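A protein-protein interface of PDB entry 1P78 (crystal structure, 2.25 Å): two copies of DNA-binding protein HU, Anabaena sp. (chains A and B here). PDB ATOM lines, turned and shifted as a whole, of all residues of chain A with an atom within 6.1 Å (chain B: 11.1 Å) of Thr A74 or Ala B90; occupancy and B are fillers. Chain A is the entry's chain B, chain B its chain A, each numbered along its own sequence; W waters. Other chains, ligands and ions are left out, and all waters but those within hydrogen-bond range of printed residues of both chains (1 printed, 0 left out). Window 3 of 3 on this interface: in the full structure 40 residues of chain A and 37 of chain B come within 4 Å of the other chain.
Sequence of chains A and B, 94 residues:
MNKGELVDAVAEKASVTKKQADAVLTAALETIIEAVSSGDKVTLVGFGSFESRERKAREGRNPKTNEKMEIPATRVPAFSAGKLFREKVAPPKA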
ATOM      1  N   SER A  37     -12.488  28.592 -17.387  1.00  0.00           N
ATOM      2  CA  SER A  37     -11.602  28.833 -18.526  1.00  0.00           C
ATOM      3  C   SER A  37     -10.282  28.040 -18.473  1.00  0.00           C
ATOM      4  O   SER A  37      -9.942  27.333 -19.412  1.00  0.00           O
ATOM      5  CB  SER A  37     -11.281  30.316 -18.667  1.00  0.00           C
ATOM      6  OG  SER A  37     -12.444  31.040 -18.995  1.00  0.00           O
ATOM      7  N   ARG A  53     -16.701  22.599 -21.576  1.00  0.00           N
ATOM      8  CA  ARG A  53     -16.966  21.388 -22.345  1.00  0.00           C
ATOM      9  C   ARG A  53     -16.534  21.521 -23.794  1.00  0.00           C
ATOM     10  O   ARG A  53     -16.794  22.547 -24.401  1.00  0.00           O
ATOM     11  CB  ARG A  53     -18.458  21.063 -22.296  1.00  0.00           C
ATOM     12  CG  ARG A  53     -18.882  20.247 -21.098  1.00  0.00           C
ATOM     13  CD  ARG A  53     -20.340  19.802 -21.233  1.00  0.00           C
ATOM     14  NE  ARG A  53     -20.970  19.328 -19.990  1.00  0.00           N
ATOM     15  CZ  ARG A  53     -22.301  19.325 -19.792  1.00  0.00           C
ATOM     16  NH1 ARG A  53     -23.140  19.786 -20.732  1.00  0.00           N
ATOM     17  NH2 ARG A  53     -22.794  18.894 -18.642  1.00  0.00           N
ATOM     18  N   GLU A  54     -15.900  20.479 -24.345  1.00  0.00           N
ATOM     19  CA  GLU A  54     -15.545  20.425 -25.775  1.00  0.00           C
ATOM     20  C   GLU A  54     -16.757  20.202 -26.677  1.00  0.00           C
ATOM     21  O   GLU A  54     -17.663  19.443 -26.364  1.00  0.00           O
ATOM     22  CB  GLU A  54     -14.483  19.376 -26.070  1.00  0.00           C
ATOM     23  CG  GLU A  54     -13.243  19.525 -25.206  1.00  0.00           C
ATOM     24  CD  GLU A  54     -12.435  20.803 -25.463  1.00  0.00           C
ATOM     25  OE1 GLU A  54     -11.667  20.868 -26.450  1.00  0.00           O
ATOM     26  OE2 GLU A  54     -12.532  21.755 -24.654  1.00  0.00           O
ATOM     27  N   ARG A  55     -16.762  20.915 -27.789  1.00  0.00           N
ATOM     28  CA  ARG A  55     -17.781  20.790 -28.816  1.00  0.00           C
ATOM     29  C   ARG A  55     -17.049  20.538 -30.120  1.00  0.00           C
ATOM     30  O   ARG A  55     -16.165  21.320 -30.494  1.00  0.00           O
ATOM     31  CB  ARG A  55     -18.545  22.120 -28.899  1.00  0.00           C
ATOM     32  CG  ARG A  55     -19.558  22.286 -27.793  1.00  0.00           C
ATOM     33  CD  ARG A  55     -20.850  21.513 -28.046  1.00  0.00           C
ATOM     34  NE  ARG A  55     -21.838  21.725 -26.974  1.00  0.00           N
ATOM     35  CZ  ARG A  55     -21.796  21.082 -25.809  1.00  0.00           C
ATOM     36  NH1 ARG A  55     -20.839  20.177 -25.585  1.00  0.00           N
ATOM     37  NH2 ARG A  55     -22.706  21.333 -24.875  1.00  0.00           N
ATOM     38  N   LYS A  56     -17.359  19.442 -30.789  1.00  0.00           N
ATOM     39  CA  LYS A  56     -16.808  19.219 -32.117  1.00  0.00           C
ATOM     40  C   LYS A  56     -17.399  20.232 -33.121  1.00  0.00           C
ATOM     41  O   LYS A  56     -18.403  20.882 -32.854  1.00  0.00           O
ATOM     42  CB  LYS A  56     -17.060  17.798 -32.603  1.00  0.00           C
ATOM     43  CG  LYS A  56     -16.561  16.672 -31.701  1.00  0.00           C
ATOM     44  CD  LYS A  56     -16.713  15.323 -32.430  1.00  0.00           C
ATOM     45  CE  LYS A  56     -16.386  14.147 -31.516  1.00  0.00           C
ATOM     46  NZ  LYS A  56     -15.097  14.312 -30.763  1.00  0.00           N
ATOM     47  N   ALA A  57     -16.710  20.389 -34.245  1.00  0.00           N
ATOM     48  CA  ALA A  57     -17.198  21.091 -35.401  1.00  0.00           C
ATOM     49  C   ALA A  57     -18.525  20.484 -35.810  1.00  0.00           C
ATOM     50  O   ALA A  57     -18.771  19.313 -35.594  1.00  0.00           O
ATOM     51  CB  ALA A  57     -16.193  20.965 -36.539  1.00  0.00           C
ATOM     52  N   PRO A  72     -16.983  25.863 -36.445  1.00  0.00           N
ATOM     53  CA  PRO A  72     -15.760  25.298 -35.863  1.00  0.00           C
ATOM     54  C   PRO A  72     -15.943  24.693 -34.474  1.00  0.00           C
ATOM     55  O   PRO A  72     -16.838  25.061 -33.714  1.00  0.00           O
ATOM     56  CB  PRO A  72     -14.828  26.503 -35.793  1.00  0.00           C
ATOM     57  CG  PRO A  72     -15.326  27.358 -36.857  1.00  0.00           C
ATOM     58  CD  PRO A  72     -16.826  27.297 -36.734  1.00  0.00           C
ATOM     59  N   ALA A  73     -15.077  23.746 -34.168  1.00  0.00           N
ATOM     60  CA  ALA A  73     -14.967  23.179 -32.834  1.00  0.00           C
ATOM     61  C   ALA A  73     -14.735  24.301 -31.813  1.00  0.00           C
ATOM     62  O   ALA A  73     -14.060  25.272 -32.091  1.00  0.00           O
ATOM     63  CB  ALA A  73     -13.817  22.175 -32.791  1.00  0.00           C
ATOM     64  N   THR A  74     -15.271  24.131 -30.618  1.00  0.00           N
ATOM     65  CA  THR A  74     -15.127  25.143 -29.593  1.00  0.00           C
ATOM     66  C   THR A  74     -15.246  24.525 -28.211  1.00  0.00           C
ATOM     67  O   THR A  74     -15.345  23.295 -28.067  1.00  0.00           O
ATOM     68  CB  THR A  74     -16.157  26.312 -29.839  1.00  0.00           C
ATOM     69  OG1 THR A  74     -15.884  27.382 -28.943  1.00  0.00           O
ATOM     70  CG2 THR A  74     -17.642  25.921 -29.566  1.00  0.00           C
ATOM     71  N   ARG A  75     -15.191  25.376 -27.201  1.00  0.00           N
ATOM     72  CA  ARG A  75     -15.409  24.977 -25.828  1.00  0.00           C
ATOM     73  C   ARG A  75     -16.473  25.914 -25.300  1.00  0.00           C
ATOM     74  O   ARG A  75     -16.412  27.112 -25.571  1.00  0.00           O
ATOM     75  CB  ARG A  75     -14.164  25.202 -24.973  1.00  0.00           C
ATOM     76  CG  ARG A  75     -12.867  24.594 -25.426  1.00  0.00           C
ATOM     77  CD  ARG A  75     -11.625  25.079 -24.594  1.00  0.00           C
ATOM     78  NE  ARG A  75     -10.373  24.582 -25.192  1.00  0.00           N
ATOM     79  CZ  ARG A  75      -9.126  24.962 -24.855  1.00  0.00           C
ATOM     80  NH1 ARG A  75      -8.892  25.860 -23.908  1.00  0.00           N
ATOM     81  NH2 ARG A  75      -8.086  24.425 -25.488  1.00  0.00           N
ATOM     82  N   VAL A  76     -17.384  25.381 -24.484  1.00  0.00           N
ATOM     83  CA  VAL A  76     -18.493  26.145 -23.917  1.00  0.00           C
ATOM     84  C   VAL A  76     -18.614  25.921 -22.385  1.00  0.00           C
ATOM     85  O   VAL A  76     -18.329  24.811 -21.873  1.00  0.00           O
ATOM     86  CB  VAL A  76     -19.828  25.797 -24.611  1.00  0.00           C
ATOM     87  CG1 VAL A  76     -19.692  25.896 -26.130  1.00  0.00           C
ATOM     88  CG2 VAL A  76     -20.280  24.398 -24.233  1.00  0.00           C
ATOM     89  N   ALA B  81     -24.940  30.825 -20.333  1.00  0.00           N
ATOM     90  CA  ALA B  81     -23.718  31.586 -20.090  1.00  0.00           C
ATOM     91  C   ALA B  81     -23.767  32.924 -20.821  1.00  0.00           C
ATOM     92  O   ALA B  81     -24.136  32.972 -21.969  1.00  0.00           O
ATOM     93  CB  ALA B  81     -22.525  30.782 -20.507  1.00  0.00           C
ATOM     94  N   GLY B  82     -23.426  34.009 -20.135  1.00  0.00           N
ATOM     95  CA  GLY B  82     -23.381  35.330 -20.751  1.00  0.00           C
ATOM     96  C   GLY B  82     -22.144  35.486 -21.623  1.00  0.00           C
ATOM     97  O   GLY B  82     -21.246  34.646 -21.573  1.00  0.00           O
ATOM     98  N   LYS B  83     -22.099  36.549 -22.420  1.00  0.00           N
ATOM     99  CA  LYS B  83     -21.058  36.726 -23.440  1.00  0.00           C
ATOM    100  C   LYS B  83     -19.604  36.728 -22.943  1.00  0.00           C
ATOM    101  O   LYS B  83     -18.756  36.085 -23.545  1.00  0.00           O
ATOM    102  CB  LYS B  83     -21.328  37.961 -24.307  1.00  0.00           C
ATOM    103  CG  LYS B  83     -20.281  38.190 -25.377  1.00  0.00           C
ATOM    104  CD  LYS B  83     -20.797  39.147 -26.434  1.00  0.00           C
ATOM    105  CE  LYS B  83     -19.686  39.595 -27.388  1.00  0.00           C
ATOM    106  NZ  LYS B  83     -20.304  40.161 -28.626  1.00  0.00           N
ATOM    107  N   LEU B  84     -19.327  37.456 -21.867  1.00  0.00           N
ATOM    108  CA  LEU B  84     -17.998  37.475 -21.256  1.00  0.00           C
ATOM    109  C   LEU B  84     -17.554  36.075 -20.851  1.00  0.00           C
ATOM    110  O   LEU B  84     -16.408  35.700 -21.079  1.00  0.00           O
ATOM    111  CB  LEU B  84     -17.919  38.426 -20.034  1.00  0.00           C
ATOM    112  CG  LEU B  84     -16.574  38.386 -19.247  1.00  0.00           C
ATOM    113  CD1 LEU B  84     -15.326  38.906 -20.074  1.00  0.00           C
ATOM    114  CD2 LEU B  84     -16.618  39.088 -17.859  1.00  0.00           C
ATOM    115  N   PHE B  85     -18.453  35.307 -20.245  1.00  0.00           N
ATOM    116  CA  PHE B  85     -18.126  33.943 -19.824  1.00  0.00           C
ATOM    117  C   PHE B  85     -17.759  33.061 -21.047  1.00  0.00           C
ATOM    118  O   PHE B  85     -16.699  32.430 -21.069  1.00  0.00           O
ATOM    119  CB  PHE B  85     -19.302  33.372 -19.015  1.00  0.00           C
ATOM    120  CG  PHE B  85     -18.956  32.166 -18.160  1.00  0.00           C
ATOM    121  CD1 PHE B  85     -17.759  31.471 -18.332  1.00  0.00           C
ATOM    122  CD2 PHE B  85     -19.868  31.709 -17.195  1.00  0.00           C
ATOM    123  CE1 PHE B  85     -17.462  30.337 -17.558  1.00  0.00           C
ATOM    124  CE2 PHE B  85     -19.582  30.589 -16.417  1.00  0.00           C
ATOM    125  CZ  PHE B  85     -18.371  29.902 -16.598  1.00  0.00           C
ATOM    126  N   ARG B  86     -18.613  33.060 -22.067  1.00  0.00           N
ATOM    127  CA  ARG B  86     -18.357  32.289 -23.287  1.00  0.00           C
ATOM    128  C   ARG B  86     -17.012  32.627 -23.953  1.00  0.00           C
ATOM    129  O   ARG B  86     -16.294  31.739 -24.426  1.00  0.00           O
ATOM    130  CB  ARG B  86     -19.481  32.461 -24.285  1.00  0.00           C
ATOM    131  CG  ARG B  86     -20.850  32.062 -23.749  1.00  0.00           C
ATOM    132  CD  ARG B  86     -21.914  31.991 -24.822  1.00  0.00           C
ATOM    133  NE  ARG B  86     -21.937  33.231 -25.597  1.00  0.00           N
ATOM    134  CZ  ARG B  86     -22.774  34.241 -25.354  1.00  0.00           C
ATOM    135  NH1 ARG B  86     -23.654  34.155 -24.363  1.00  0.00           N
ATOM    136  NH2 ARG B  86     -22.739  35.340 -26.105  1.00  0.00           N
ATOM    137  N   GLU B  87     -16.676  33.910 -23.946  1.00  0.00           N
ATOM    138  CA  GLU B  87     -15.503  34.392 -24.626  1.00  0.00           C
ATOM    139  C   GLU B  87     -14.214  34.168 -23.857  1.00  0.00           C
ATOM    140  O   GLU B  87     -13.164  34.118 -24.454  1.00  0.00           O
ATOM    141  CB  GLU B  87     -15.689  35.835 -25.057  1.00  0.00           C
ATOM    142  CG  GLU B  87     -16.659  35.926 -26.233  1.00  0.00           C
ATOM    143  CD  GLU B  87     -16.808  37.331 -26.798  1.00  0.00           C
ATOM    144  OE1 GLU B  87     -17.416  37.469 -27.895  1.00  0.00           O
ATOM    145  OE2 GLU B  87     -16.329  38.293 -26.141  1.00  0.00           O
ATOM    146  N   LYS B  88     -14.297  33.979 -22.547  1.00  0.00           N
ATOM    147  CA  LYS B  88     -13.127  33.563 -21.779  1.00  0.00           C
ATOM    148  C   LYS B  88     -12.881  32.069 -21.924  1.00  0.00           C
ATOM    149  O   LYS B  88     -11.749  31.619 -21.815  1.00  0.00           O
ATOM    150  CB  LYS B  88     -13.271  33.881 -20.292  1.00  0.00           C
ATOM    151  CG  LYS B  88     -13.442  35.358 -19.953  1.00  0.00           C
ATOM    152  CD  LYS B  88     -12.328  36.191 -20.520  1.00  0.00           C
ATOM    153  CE  LYS B  88     -11.128  36.225 -19.579  1.00  0.00           C
ATOM    154  NZ  LYS B  88     -11.385  36.956 -18.305  1.00  0.00           N
ATOM    155  N   VAL B  89     -13.946  31.302 -22.123  1.00  0.00           N
ATOM    156  CA  VAL B  89     -13.813  29.868 -22.291  1.00  0.00           C
ATOM    157  C   VAL B  89     -13.310  29.586 -23.710  1.00  0.00           C
ATOM    158  O   VAL B  89     -12.454  28.715 -23.919  1.00  0.00           O
ATOM    159  CB  VAL B  89     -15.152  29.147 -21.974  1.00  0.00           C
ATOM    160  CG1 VAL B  89     -15.157  27.707 -22.450  1.00  0.00           C
ATOM    161  CG2 VAL B  89     -15.423  29.197 -20.499  1.00  0.00           C
ATOM    162  N   ALA B  90     -13.821  30.349 -24.671  1.00  0.00           N
ATOM    163  CA  ALA B  90     -13.356  30.270 -26.048  1.00  0.00           C
ATOM    164  C   ALA B  90     -13.117  31.669 -26.631  1.00  0.00           C
ATOM    165  O   ALA B  90     -14.022  32.291 -27.218  1.00  0.00           O
ATOM    166  CB  ALA B  90     -14.329  29.476 -26.895  1.00  0.00           C
ATOM    167  N   PRO B  91     -11.901  32.175 -26.411  1.00  0.00           N
ATOM    168  CA  PRO B  91     -11.458  33.453 -26.988  1.00  0.00           C
ATOM    169  C   PRO B  91     -11.681  33.512 -28.503  1.00  0.00           C
ATOM    170  O   PRO B  91     -11.186  32.652 -29.248  1.00  0.00           O
ATOM    171  CB  PRO B  91      -9.960  33.494 -26.649  1.00  0.00           C
ATOM    172  CG  PRO B  91      -9.830  32.636 -25.405  1.00  0.00           C
ATOM    173  CD  PRO B  91     -10.882  31.571 -25.532  1.00  0.00           C
ATOM    174  N   PRO B  92     -12.434  34.509 -28.958  1.00  0.00           N
ATOM    175  CA  PRO B  92     -12.699  34.689 -30.394  1.00  0.00           C
ATOM    176  C   PRO B  92     -11.429  35.036 -31.187  1.00  0.00           C
ATOM    177  O   PRO B  92     -10.483  35.578 -30.602  1.00  0.00           O
ATOM    178  CB  PRO B  92     -13.685  35.871 -30.417  1.00  0.00           C
ATOM    179  CG  PRO B  92     -14.285  35.875 -29.033  1.00  0.00           C
ATOM    180  CD  PRO B  92     -13.114  35.531 -28.136  1.00  0.00           C
HETATM  181  O   HOH W   1     -17.621  29.387 -24.908  1.00  0.00           O
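O of Lys B88 lies within hydrogen-bond range of OG of Ser A37 (3.0 Å). The side-chain hydroxyl (OG) of Ser A37 is in hydrogen-bond range of the backbone NH (N) of Val B89 (3.5 Å).
N of Arg A53 sits at hydrogen-bond distance from O of Val A76 (2.8 Å). OE2 of Glu A54 is in salt-bridge range of NE of Arg A75 (3.6 Å). O of Thr A74 is in hydrogen-bond range of N of Arg A55 (2.8 Å).
Among the printed residues, pairs that only touch across the chains: Thr A74 with Ala B90 (3.3 Å), Arg A75 with Val B89 (3.4 Å), Arg A75 with Ala B90 (3.4 Å) and Val A76 with Val B89 (3.8 Å).
Of the printed residues of chain B, Ser A37 touches Lys B88 (3.0 Å) and Val B89 (3.5 Å). No residue of chain B comes within 4 Å of Glu A54. No residue of chain B comes within 4 Å of Pro A72. No residue of chain B comes within 4 Å of Ala A73. Thr A74 touches just one residue of chain B: Ala B90. Of the printed residues of chain B, Arg A75 touches Val B89 (3.4 Å) and Ala B90 (3.4 Å). Of chain B, only Val B89 (3.8 Å) comes within 4 Å of Val A76. Arg B86 touches none of the printed residues of chain A. Of the printed residues of chain A, Lys B88 touches Ser A37 (3.0 Å). Of chain A, only Thr A74 and Arg A75 come within 4 Å of Ala B90.
Printed residues of chain A that touch a printed residue of chain B: Ser A37, Thr A74, Arg A75 and Val A76. Of the 12 printed residues of chain B, 3 touch a printed residue of chain A. Hydrophobic or aromatic side chains of chain B that line the printed part of chain A: Val B89 and Ala B90.
No position is printed for both chains. Of the 6 pairs that touch across the chains among the printed residues, none has its exchanged pair printed and touching as well.
Water W1 bridges O of Arg A75 (2.7 Å) and O of Arg B86 (2.7 Å).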
